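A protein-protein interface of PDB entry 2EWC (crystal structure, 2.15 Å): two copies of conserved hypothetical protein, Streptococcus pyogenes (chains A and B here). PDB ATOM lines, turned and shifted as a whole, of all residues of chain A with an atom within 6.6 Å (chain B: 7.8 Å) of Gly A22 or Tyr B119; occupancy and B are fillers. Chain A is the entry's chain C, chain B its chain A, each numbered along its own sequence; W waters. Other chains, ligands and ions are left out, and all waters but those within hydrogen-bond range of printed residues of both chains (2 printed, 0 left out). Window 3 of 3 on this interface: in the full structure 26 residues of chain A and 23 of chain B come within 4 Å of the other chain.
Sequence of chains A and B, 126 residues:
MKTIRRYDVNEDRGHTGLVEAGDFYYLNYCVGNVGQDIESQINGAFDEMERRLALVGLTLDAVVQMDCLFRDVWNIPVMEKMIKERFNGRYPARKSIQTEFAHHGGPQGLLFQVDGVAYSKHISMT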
ATOM      1  N   THR A   3     -35.323  14.442 -29.177  1.00  0.00           N
ATOM      2  CA  THR A   3     -34.579  14.658 -30.446  1.00  0.00           C
ATOM      3  C   THR A   3     -33.114  14.249 -30.257  1.00  0.00           C
ATOM      4  O   THR A   3     -32.452  13.866 -31.226  1.00  0.00           O
ATOM      5  CB  THR A   3     -34.625  16.152 -30.925  1.00  0.00           C
ATOM      6  OG1 THR A   3     -35.900  16.751 -30.631  1.00  0.00           O
ATOM      7  CG2 THR A   3     -34.348  16.265 -32.441  1.00  0.00           C
ATOM      8  N   ILE A   4     -32.595  14.325 -29.033  1.00  0.00           N
ATOM      9  CA  ILE A   4     -31.207  13.909 -28.802  1.00  0.00           C
ATOM     10  C   ILE A   4     -31.076  12.366 -28.761  1.00  0.00           C
ATOM     11  O   ILE A   4     -31.808  11.691 -28.025  1.00  0.00           O
ATOM     12  CB  ILE A   4     -30.620  14.542 -27.512  1.00  0.00           C
ATOM     13  CG1 ILE A   4     -30.650  16.073 -27.595  1.00  0.00           C
ATOM     14  CG2 ILE A   4     -29.198  14.064 -27.290  1.00  0.00           C
ATOM     15  CD1 ILE A   4     -30.181  16.811 -26.315  1.00  0.00           C
ATOM     16  N   GLU A  20     -25.750  12.401 -30.620  1.00  0.00           N
ATOM     17  CA  GLU A  20     -26.278  12.927 -31.852  1.00  0.00           C
ATOM     18  C   GLU A  20     -27.259  14.033 -31.527  1.00  0.00           C
ATOM     19  O   GLU A  20     -28.249  13.806 -30.822  1.00  0.00           O
ATOM     20  CB  GLU A  20     -27.016  11.810 -32.618  1.00  0.00           C
ATOM     21  CG  GLU A  20     -27.662  12.271 -33.935  1.00  0.00           C
ATOM     22  CD  GLU A  20     -28.482  11.152 -34.643  1.00  0.00           C
ATOM     23  OE1 GLU A  20     -28.269   9.956 -34.389  1.00  0.00           O
ATOM     24  OE2 GLU A  20     -29.351  11.475 -35.462  1.00  0.00           O
ATOM     25  N   ALA A  21     -26.967  15.228 -32.029  1.00  0.00           N
ATOM     26  CA  ALA A  21     -27.779  16.433 -31.797  1.00  0.00           C
ATOM     27  C   ALA A  21     -27.991  17.127 -33.134  1.00  0.00           C
ATOM     28  O   ALA A  21     -27.155  17.919 -33.587  1.00  0.00           O
ATOM     29  CB  ALA A  21     -27.075  17.362 -30.823  1.00  0.00           C
ATOM     30  N   GLY A  22     -29.090  16.788 -33.787  1.00  0.00           N
ATOM     31  CA  GLY A  22     -29.381  17.321 -35.108  1.00  0.00           C
ATOM     32  C   GLY A  22     -28.401  16.746 -36.110  1.00  0.00           C
ATOM     33  O   GLY A  22     -28.266  15.516 -36.247  1.00  0.00           O
ATOM     34  N   ASP A  23     -27.694  17.647 -36.782  1.00  0.00           N
ATOM     35  CA  ASP A  23     -26.629  17.292 -37.746  1.00  0.00           C
ATOM     36  C   ASP A  23     -25.238  17.117 -37.119  1.00  0.00           C
ATOM     37  O   ASP A  23     -24.261  16.818 -37.806  1.00  0.00           O
ATOM     38  CB  ASP A  23     -26.547  18.366 -38.824  1.00  0.00           C
ATOM     39  CG  ASP A  23     -27.775  18.406 -39.708  1.00  0.00           C
ATOM     40  OD1 ASP A  23     -28.515  17.400 -39.823  1.00  0.00           O
ATOM     41  OD2 ASP A  23     -27.991  19.477 -40.299  1.00  0.00           O
ATOM     42  N   PHE A  24     -25.159  17.277 -35.808  1.00  0.00           N
ATOM     43  CA  PHE A  24     -23.881  17.240 -35.097  1.00  0.00           C
ATOM     44  C   PHE A  24     -23.763  16.093 -34.136  1.00  0.00           C
ATOM     45  O   PHE A  24     -24.756  15.666 -33.561  1.00  0.00           O
ATOM     46  CB  PHE A  24     -23.618  18.562 -34.366  1.00  0.00           C
ATOM     47  CG  PHE A  24     -23.284  19.659 -35.278  1.00  0.00           C
ATOM     48  CD1 PHE A  24     -21.966  19.904 -35.620  1.00  0.00           C
ATOM     49  CD2 PHE A  24     -24.299  20.414 -35.881  1.00  0.00           C
ATOM     50  CE1 PHE A  24     -21.651  20.921 -36.510  1.00  0.00           C
ATOM     51  CE2 PHE A  24     -23.998  21.441 -36.773  1.00  0.00           C
ATOM     52  CZ  PHE A  24     -22.674  21.707 -37.078  1.00  0.00           C
ATOM     53  N   TYR A  25     -22.534  15.597 -33.987  1.00  0.00           N
ATOM     54  CA  TYR A  25     -22.238  14.416 -33.198  1.00  0.00           C
ATOM     55  C   TYR A  25     -21.095  14.771 -32.285  1.00  0.00           C
ATOM     56  O   TYR A  25     -20.062  15.164 -32.769  1.00  0.00           O
ATOM     57  CB  TYR A  25     -21.842  13.237 -34.111  1.00  0.00           C
ATOM     58  CG  TYR A  25     -22.951  12.869 -35.062  1.00  0.00           C
ATOM     59  CD1 TYR A  25     -23.814  11.818 -34.773  1.00  0.00           C
ATOM     60  CD2 TYR A  25     -23.175  13.612 -36.220  1.00  0.00           C
ATOM     61  CE1 TYR A  25     -24.858  11.491 -35.637  1.00  0.00           C
ATOM     62  CE2 TYR A  25     -24.211  13.311 -37.087  1.00  0.00           C
ATOM     63  CZ  TYR A  25     -25.053  12.245 -36.792  1.00  0.00           C
ATOM     64  OH  TYR A  25     -26.099  11.935 -37.640  1.00  0.00           O
ATOM     65  N   TYR A  26     -21.285  14.605 -30.980  1.00  0.00           N
ATOM     66  CA  TYR A  26     -20.271  14.941 -30.002  1.00  0.00           C
ATOM     67  C   TYR A  26     -19.727  13.650 -29.447  1.00  0.00           C
ATOM     68  O   TYR A  26     -20.470  12.823 -28.947  1.00  0.00           O
ATOM     69  CB  TYR A  26     -20.844  15.845 -28.890  1.00  0.00           C
ATOM     70  CG  TYR A  26     -21.242  17.190 -29.446  1.00  0.00           C
ATOM     71  CD1 TYR A  26     -20.412  18.290 -29.311  1.00  0.00           C
ATOM     72  CD2 TYR A  26     -22.424  17.337 -30.173  1.00  0.00           C
ATOM     73  CE1 TYR A  26     -20.755  19.499 -29.829  1.00  0.00           C
ATOM     74  CE2 TYR A  26     -22.774  18.540 -30.711  1.00  0.00           C
ATOM     75  CZ  TYR A  26     -21.939  19.622 -30.539  1.00  0.00           C
ATOM     76  OH  TYR A  26     -22.307  20.849 -31.081  1.00  0.00           O
ATOM     77  N   SER A 120     -22.890  15.542 -40.062  1.00  0.00           N
ATOM     78  CA  SER A 120     -23.528  14.900 -41.207  1.00  0.00           C
ATOM     79  C   SER A 120     -24.876  15.578 -41.455  1.00  0.00           C
ATOM     80  O   SER A 120     -25.739  15.607 -40.571  1.00  0.00           O
ATOM     81  CB  SER A 120     -23.718  13.398 -40.969  1.00  0.00           C
ATOM     82  OG  SER A 120     -24.089  12.744 -42.164  1.00  0.00           O
ATOM     83  N   HIS A 122     -28.467  16.057 -42.383  1.00  0.00           N
ATOM     84  CA  HIS A 122     -29.749  15.411 -42.605  1.00  0.00           C
ATOM     85  C   HIS A 122     -30.627  16.355 -43.405  1.00  0.00           C
ATOM     86  O   HIS A 122     -31.282  15.918 -44.347  1.00  0.00           O
ATOM     87  CB  HIS A 122     -30.431  15.070 -41.276  1.00  0.00           C
ATOM     88  CG  HIS A 122     -29.616  14.170 -40.403  1.00  0.00           C
ATOM     89  ND1 HIS A 122     -29.797  12.800 -40.365  1.00  0.00           N
ATOM     90  CD2 HIS A 122     -28.602  14.439 -39.551  1.00  0.00           C
ATOM     91  CE1 HIS A 122     -28.928  12.268 -39.525  1.00  0.00           C
ATOM     92  NE2 HIS A 122     -28.193  13.242 -39.015  1.00  0.00           N
ATOM     93  N   ALA B  21     -27.163  29.990 -30.367  1.00  0.00           N
ATOM     94  CA  ALA B  21     -26.941  30.026 -31.816  1.00  0.00           C
ATOM     95  C   ALA B  21     -27.705  28.911 -32.543  1.00  0.00           C
ATOM     96  O   ALA B  21     -27.271  27.735 -32.566  1.00  0.00           O
ATOM     97  CB  ALA B  21     -25.466  29.926 -32.125  1.00  0.00           C
ATOM     98  N   GLY B  22     -28.842  29.271 -33.140  1.00  0.00           N
ATOM     99  CA  GLY B  22     -29.710  28.296 -33.782  1.00  0.00           C
ATOM    100  C   GLY B  22     -30.278  27.320 -32.756  1.00  0.00           C
ATOM    101  O   GLY B  22     -30.886  27.740 -31.760  1.00  0.00           O
ATOM    102  N   ASP B  23     -30.052  26.027 -32.986  1.00  0.00           N
ATOM    103  CA  ASP B  23     -30.495  24.969 -32.058  1.00  0.00           C
ATOM    104  C   ASP B  23     -29.482  24.629 -30.948  1.00  0.00           C
ATOM    105  O   ASP B  23     -29.726  23.740 -30.117  1.00  0.00           O
ATOM    106  CB  ASP B  23     -30.828  23.686 -32.828  1.00  0.00           C
ATOM    107  CG  ASP B  23     -32.078  23.813 -33.698  1.00  0.00           C
ATOM    108  OD1 ASP B  23     -32.943  24.674 -33.440  1.00  0.00           O
ATOM    109  OD2 ASP B  23     -32.188  23.025 -34.645  1.00  0.00           O
ATOM    110  N   PHE B  24     -28.366  25.341 -30.944  1.00  0.00           N
ATOM    111  CA  PHE B  24     -27.259  25.118 -30.016  1.00  0.00           C
ATOM    112  C   PHE B  24     -27.049  26.253 -29.014  1.00  0.00           C
ATOM    113  O   PHE B  24     -27.318  27.414 -29.322  1.00  0.00           O
ATOM    114  CB  PHE B  24     -25.993  24.824 -30.812  1.00  0.00           C
ATOM    115  CG  PHE B  24     -26.013  23.451 -31.459  1.00  0.00           C
ATOM    116  CD1 PHE B  24     -25.525  22.345 -30.774  1.00  0.00           C
ATOM    117  CD2 PHE B  24     -26.573  23.266 -32.721  1.00  0.00           C
ATOM    118  CE1 PHE B  24     -25.571  21.094 -31.317  1.00  0.00           C
ATOM    119  CE2 PHE B  24     -26.611  21.997 -33.299  1.00  0.00           C
ATOM    120  CZ  PHE B  24     -26.107  20.911 -32.605  1.00  0.00           C
ATOM    121  N   TYR B  25     -26.608  25.879 -27.806  1.00  0.00           N
ATOM    122  CA  TYR B  25     -26.437  26.775 -26.683  1.00  0.00           C
ATOM    123  C   TYR B  25     -25.027  26.528 -26.110  1.00  0.00           C
ATOM    124  O   TYR B  25     -24.654  25.389 -25.798  1.00  0.00           O
ATOM    125  CB  TYR B  25     -27.504  26.527 -25.620  1.00  0.00           C
ATOM    126  CG  TYR B  25     -28.938  26.740 -26.095  1.00  0.00           C
ATOM    127  CD1 TYR B  25     -29.618  27.948 -25.856  1.00  0.00           C
ATOM    128  CD2 TYR B  25     -29.612  25.732 -26.797  1.00  0.00           C
ATOM    129  CE1 TYR B  25     -30.938  28.127 -26.314  1.00  0.00           C
ATOM    130  CE2 TYR B  25     -30.896  25.907 -27.251  1.00  0.00           C
ATOM    131  CZ  TYR B  25     -31.564  27.099 -27.002  1.00  0.00           C
ATOM    132  OH  TYR B  25     -32.856  27.228 -27.466  1.00  0.00           O
ATOM    133  N   TYR B  26     -24.241  27.598 -26.001  1.00  0.00           N
ATOM    134  CA  TYR B  26     -22.858  27.492 -25.546  1.00  0.00           C
ATOM    135  C   TYR B  26     -22.754  28.127 -24.199  1.00  0.00           C
ATOM    136  O   TYR B  26     -23.001  29.313 -24.052  1.00  0.00           O
ATOM    137  CB  TYR B  26     -21.906  28.167 -26.544  1.00  0.00           C
ATOM    138  CG  TYR B  26     -21.826  27.365 -27.810  1.00  0.00           C
ATOM    139  CD1 TYR B  26     -20.808  26.425 -28.010  1.00  0.00           C
ATOM    140  CD2 TYR B  26     -22.819  27.474 -28.786  1.00  0.00           C
ATOM    141  CE1 TYR B  26     -20.767  25.647 -29.168  1.00  0.00           C
ATOM    142  CE2 TYR B  26     -22.775  26.685 -29.956  1.00  0.00           C
ATOM    143  CZ  TYR B  26     -21.747  25.783 -30.128  1.00  0.00           C
ATOM    144  OH  TYR B  26     -21.715  25.002 -31.283  1.00  0.00           O
ATOM    145  N   LEU B  27     -22.430  27.313 -23.207  1.00  0.00           N
ATOM    146  CA  LEU B  27     -22.229  27.790 -21.864  1.00  0.00           C
ATOM    147  C   LEU B  27     -20.785  28.239 -21.660  1.00  0.00           C
ATOM    148  O   LEU B  27     -19.838  27.540 -22.063  1.00  0.00           O
ATOM    149  CB  LEU B  27     -22.598  26.676 -20.892  1.00  0.00           C
ATOM    150  CG  LEU B  27     -24.125  26.462 -20.804  1.00  0.00           C
ATOM    151  CD1 LEU B  27     -24.557  24.989 -20.958  1.00  0.00           C
ATOM    152  CD2 LEU B  27     -24.664  27.050 -19.545  1.00  0.00           C
ATOM    153  N   LEU B  53     -29.203  27.463 -18.083  1.00  0.00           N
ATOM    154  CA  LEU B  53     -30.099  26.735 -18.971  1.00  0.00           C
ATOM    155  C   LEU B  53     -31.546  27.121 -18.729  1.00  0.00           C
ATOM    156  O   LEU B  53     -32.322  27.146 -19.675  1.00  0.00           O
ATOM    157  CB  LEU B  53     -29.910  25.221 -18.865  1.00  0.00           C
ATOM    158  CG  LEU B  53     -28.560  24.709 -19.395  1.00  0.00           C
ATOM    159  CD1 LEU B  53     -28.351  23.226 -19.030  1.00  0.00           C
ATOM    160  CD2 LEU B  53     -28.434  24.936 -20.907  1.00  0.00           C
ATOM    161  N   LEU B  58     -34.531  25.386 -20.487  1.00  0.00           N
ATOM    162  CA  LEU B  58     -33.891  24.092 -20.670  1.00  0.00           C
ATOM    163  C   LEU B  58     -33.352  23.521 -19.364  1.00  0.00           C
ATOM    164  O   LEU B  58     -33.161  24.242 -18.374  1.00  0.00           O
ATOM    165  CB  LEU B  58     -32.773  24.193 -21.724  1.00  0.00           C
ATOM    166  CG  LEU B  58     -33.226  24.635 -23.122  1.00  0.00           C
ATOM    167  CD1 LEU B  58     -32.036  24.724 -24.051  1.00  0.00           C
ATOM    168  CD2 LEU B  58     -34.312  23.679 -23.695  1.00  0.00           C
ATOM    169  N   THR B  59     -33.078  22.218 -19.387  1.00  0.00           N
ATOM    170  CA  THR B  59     -32.590  21.489 -18.221  1.00  0.00           C
ATOM    171  C   THR B  59     -31.303  20.743 -18.613  1.00  0.00           C
ATOM    172  O   THR B  59     -30.858  20.830 -19.769  1.00  0.00           O
ATOM    173  CB  THR B  59     -33.666  20.491 -17.717  1.00  0.00           C
ATOM    174  OG1 THR B  59     -33.811  19.421 -18.664  1.00  0.00           O
ATOM    175  CG2 THR B  59     -35.059  21.185 -17.521  1.00  0.00           C
ATOM    176  N   ASP B  61     -31.012  17.755 -19.215  1.00  0.00           N
ATOM    177  CA  ASP B  61     -31.396  16.844 -20.287  1.00  0.00           C
ATOM    178  C   ASP B  61     -30.919  17.295 -21.665  1.00  0.00           C
ATOM    179  O   ASP B  61     -30.696  16.455 -22.545  1.00  0.00           O
ATOM    180  CB  ASP B  61     -32.921  16.700 -20.346  1.00  0.00           C
ATOM    181  CG  ASP B  61     -33.427  15.531 -19.531  1.00  0.00           C
ATOM    182  OD1 ASP B  61     -34.259  15.759 -18.605  1.00  0.00           O
ATOM    183  OD2 ASP B  61     -33.002  14.380 -19.826  1.00  0.00           O
ATOM    184  N   ALA B  62     -30.792  18.614 -21.840  1.00  0.00           N
ATOM    185  CA  ALA B  62     -30.435  19.207 -23.137  1.00  0.00           C
ATOM    186  C   ALA B  62     -28.909  19.311 -23.371  1.00  0.00           C
ATOM    187  O   ALA B  62     -28.471  19.655 -24.453  1.00  0.00           O
ATOM    188  CB  ALA B  62     -31.089  20.562 -23.273  1.00  0.00           C
ATOM    189  N   VAL B  63     -28.112  19.025 -22.353  1.00  0.00           N
ATOM    190  CA  VAL B  63     -26.652  19.133 -22.465  1.00  0.00           C
ATOM    191  C   VAL B  63     -26.074  17.953 -23.278  1.00  0.00           C
ATOM    192  O   VAL B  63     -26.306  16.766 -22.951  1.00  0.00           O
ATOM    193  CB  VAL B  63     -25.990  19.167 -21.095  1.00  0.00           C
ATOM    194  CG1 VAL B  63     -24.460  19.160 -21.260  1.00  0.00           C
ATOM    195  CG2 VAL B  63     -26.439  20.433 -20.287  1.00  0.00           C
ATOM    196  N   VAL B  64     -25.340  18.278 -24.337  1.00  0.00           N
ATOM    197  CA  VAL B  64     -24.751  17.247 -25.189  1.00  0.00           C
ATOM    198  C   VAL B  64     -23.263  16.991 -24.968  1.00  0.00           C
ATOM    199  O   VAL B  64     -22.772  15.905 -25.292  1.00  0.00           O
ATOM    200  CB  VAL B  64     -25.050  17.506 -26.706  1.00  0.00           C
ATOM    201  CG1 VAL B  64     -26.579  17.481 -26.946  1.00  0.00           C
ATOM    202  CG2 VAL B  64     -24.417  18.782 -27.207  1.00  0.00           C
ATOM    203  N   GLN B  65     -22.557  17.986 -24.425  1.00  0.00           N
ATOM    204  CA  GLN B  65     -21.114  17.931 -24.274  1.00  0.00           C
ATOM    205  C   GLN B  65     -20.689  18.845 -23.139  1.00  0.00           C
ATOM    206  O   GLN B  65     -21.238  19.930 -22.996  1.00  0.00           O
ATOM    207  CB  GLN B  65     -20.386  18.301 -25.585  1.00  0.00           C
ATOM    208  CG  GLN B  65     -18.927  17.868 -25.611  1.00  0.00           C
ATOM    209  CD  GLN B  65     -18.014  18.890 -24.941  1.00  0.00           C
ATOM    210  OE1 GLN B  65     -18.336  20.087 -24.899  1.00  0.00           O
ATOM    211  NE2 GLN B  65     -16.900  18.418 -24.355  1.00  0.00           N
ATOM    212  N   VAL B 117     -22.087  22.463 -24.009  1.00  0.00           N
ATOM    213  CA  VAL B 117     -22.926  22.752 -25.147  1.00  0.00           C
ATOM    214  C   VAL B 117     -24.227  22.013 -24.896  1.00  0.00           C
ATOM    215  O   VAL B 117     -24.230  20.823 -24.512  1.00  0.00           O
ATOM    216  CB  VAL B 117     -22.298  22.251 -26.493  1.00  0.00           C
ATOM    217  CG1 VAL B 117     -23.178  22.607 -27.661  1.00  0.00           C
ATOM    218  CG2 VAL B 117     -20.882  22.802 -26.705  1.00  0.00           C
ATOM    219  N   ALA B 118     -25.326  22.724 -25.095  1.00  0.00           N
ATOM    220  CA  ALA B 118     -26.638  22.128 -25.001  1.00  0.00           C
ATOM    221  C   ALA B 118     -27.362  22.278 -26.349  1.00  0.00           C
ATOM    222  O   ALA B 118     -26.986  23.114 -27.167  1.00  0.00           O
ATOM    223  CB  ALA B 118     -27.437  22.783 -23.854  1.00  0.00           C
ATOM    224  N   TYR B 119     -28.395  21.469 -26.560  1.00  0.00           N
ATOM    225  CA  TYR B 119     -29.101  21.414 -27.833  1.00  0.00           C
ATOM    226  C   TYR B 119     -30.610  21.378 -27.607  1.00  0.00           C
ATOM    227  O   TYR B 119     -31.099  20.674 -26.700  1.00  0.00           O
ATOM    228  CB  TYR B 119     -28.689  20.151 -28.589  1.00  0.00           C
ATOM    229  CG  TYR B 119     -29.491  19.883 -29.846  1.00  0.00           C
ATOM    230  CD1 TYR B 119     -29.181  20.542 -31.021  1.00  0.00           C
ATOM    231  CD2 TYR B 119     -30.553  18.960 -29.850  1.00  0.00           C
ATOM    232  CE1 TYR B 119     -29.876  20.322 -32.154  1.00  0.00           C
ATOM    233  CE2 TYR B 119     -31.282  18.726 -30.994  1.00  0.00           C
ATOM    234  CZ  TYR B 119     -30.927  19.409 -32.152  1.00  0.00           C
ATOM    235  OH  TYR B 119     -31.616  19.224 -33.314  1.00  0.00           O
ATOM    236  N   SER B 120     -31.343  22.144 -28.411  1.00  0.00           N
ATOM    237  CA  SER B 120     -32.809  22.071 -28.417  1.00  0.00           C
ATOM    238  C   SER B 120     -33.318  22.479 -29.788  1.00  0.00           C
ATOM    239  O   SER B 120     -33.088  23.603 -30.234  1.00  0.00           O
ATOM    240  CB  SER B 120     -33.440  22.958 -27.343  1.00  0.00           C
ATOM    241  OG  SER B 120     -34.807  22.618 -27.169  1.00  0.00           O
ATOM    242  N   LYS B 121     -33.985  21.540 -30.455  1.00  0.00           N
ATOM    243  CA  LYS B 121     -34.490  21.742 -31.814  1.00  0.00           C
ATOM    244  C   LYS B 121     -35.690  22.694 -31.796  1.00  0.00           C
ATOM    245  O   LYS B 121     -36.670  22.443 -31.094  1.00  0.00           O
ATOM    246  CB  LYS B 121     -34.853  20.390 -32.431  1.00  0.00           C
ATOM    247  CG  LYS B 121     -35.705  20.446 -33.677  1.00  0.00           C
ATOM    248  CD  LYS B 121     -34.950  19.992 -34.901  1.00  0.00           C
ATOM    249  CE  LYS B 121     -34.653  21.157 -35.830  1.00  0.00           C
ATOM    250  NZ  LYS B 121     -34.625  20.655 -37.247  1.00  0.00           N
ATOM    251  N   HIS B 122     -35.577  23.794 -32.546  1.00  0.00           N
ATOM    252  CA  HIS B 122     -36.648  24.796 -32.653  1.00  0.00           C
ATOM    253  C   HIS B 122     -37.630  24.410 -33.751  1.00  0.00           C
ATOM    254  O   HIS B 122     -37.227  23.835 -34.757  1.00  0.00           O
ATOM    255  CB  HIS B 122     -36.073  26.194 -32.935  1.00  0.00           C
ATOM    256  CG  HIS B 122     -35.296  26.764 -31.793  1.00  0.00           C
ATOM    257  ND1 HIS B 122     -35.767  27.800 -31.015  1.00  0.00           N
ATOM    258  CD2 HIS B 122     -34.085  26.432 -31.285  1.00  0.00           C
ATOM    259  CE1 HIS B 122     -34.879  28.084 -30.080  1.00  0.00           C
ATOM    260  NE2 HIS B 122     -33.848  27.267 -30.222  1.00  0.00           N
HETATM  261  O   HOH W   1     -34.805  18.814 -29.240  1.00  0.00           O
HETATM  262  O   HOH W   2     -20.248  22.770 -31.452  1.00  0.00           O
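Among the printed residues, pairs that only touch across the chains: Tyr A26 with Phe B24 (3.3 Å), Ala A21 with Phe B24 (3.3 Å), Gly A22 with Tyr B119 (3.4 Å), Ala A21 with Tyr B119 (3.6 Å), Ile A4 with Tyr B119 (3.7 Å), Ile A4 with Val B64 (3.7 Å), Tyr A26 with Gln B65 (3.7 Å), Phe A24 with Phe B24 (3.8 Å), Ile A4 with Ala B62 (3.8 Å), Ile A4 with Asp B61 (3.8 Å), Tyr A26 with Val B64 (3.9 Å), Ala A21 with Val B64 (3.9 Å) and Tyr A26 with Val B117 (3.9 Å).
Ala A21 touches Phe B24, but with the chains exchanged Phe A24 does not touch Ala B21 (8.2 Å). Phe B24 touches its own counterpart, Phe A24. Tyr A26 touches Phe B24, but with the chains exchanged Phe A24 does not touch Tyr B26 (6.6 Å). 8 positions are printed for both chains.
Printed residues of chain B that touch a printed residue of chain A: Phe B24, Asp B61, Ala B62, Val B64, Gln B65, Val B117 and Tyr B119. Hydrophobic or aromatic side chains of chain B that line the printed part of chain A: Phe B24, Val B64, Val B117 and Tyr B119. Of the 11 printed residues of chain A, 5 touch a printed residue of chain B. Along chain A the printed residues that touch a printed residue of chain B span positions 4 to 26. Among the printed residues, 13 pairs touch across the chains. Among the printed residues, no Asp or Glu carboxylate lies within 4 Å of a Lys or Arg side-chain nitrogen of the other chain.
Of the printed residues of chain B, Ile A4 touches Asp B61 (3.8 Å), Ala B62 (3.8 Å), Val B64 (3.7 Å) and Tyr B119 (3.7 Å). Ala A21 touches just these residues of chain B: Phe B24 (3.3 Å), Val B64 (3.9 Å) and Tyr B119 (3.6 Å). Gly A22 touches just one residue of chain B: Tyr B119. Tyr A25 touches none of the printed residues of chain B. Of the printed residues of chain B, Tyr A26 touches Phe B24, Val B64, Gln B65 and Val B117. Thr B59 touches none of the printed residues of chain A. Of the printed residues of chain A, Val B64 touches Ile A4, Ala A21 and Tyr A26. Of the printed residues of chain A, Gln B65 touches Tyr A26 (3.7 Å). The nearest residue of chain A that does not touch Tyr B119 is Thr A3 (4.1 Å).
Water W2 lies within hydrogen-bond range of OH of Tyr B26 (2.7 Å) and OH of Tyr A26 (2.8 Å). Water W1 lies within hydrogen-bond range of the side-chain hydroxyl (OG1) of Thr A3 (2.7 Å) and the backbone NH (N) of Lys B121 (3.1 Å).
The side-chain hydroxyl (OG1) of Thr B59 lies close to the backbone NH (N) of Asp B61, 3.3 Å away. The backbone NH (N) of Tyr B119 is in hydrogen-bond range of the backbone carbonyl oxygen (O) of Ala B62, at 2.8 Å. The backbone NH (N) of Val B64 sits at hydrogen-bond distance from the backbone carbonyl oxygen (O) of Val B117, at 2.8 Å. O of Gln B65 is in hydrogen-bond range of N of Val B117 (2.9 Å).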
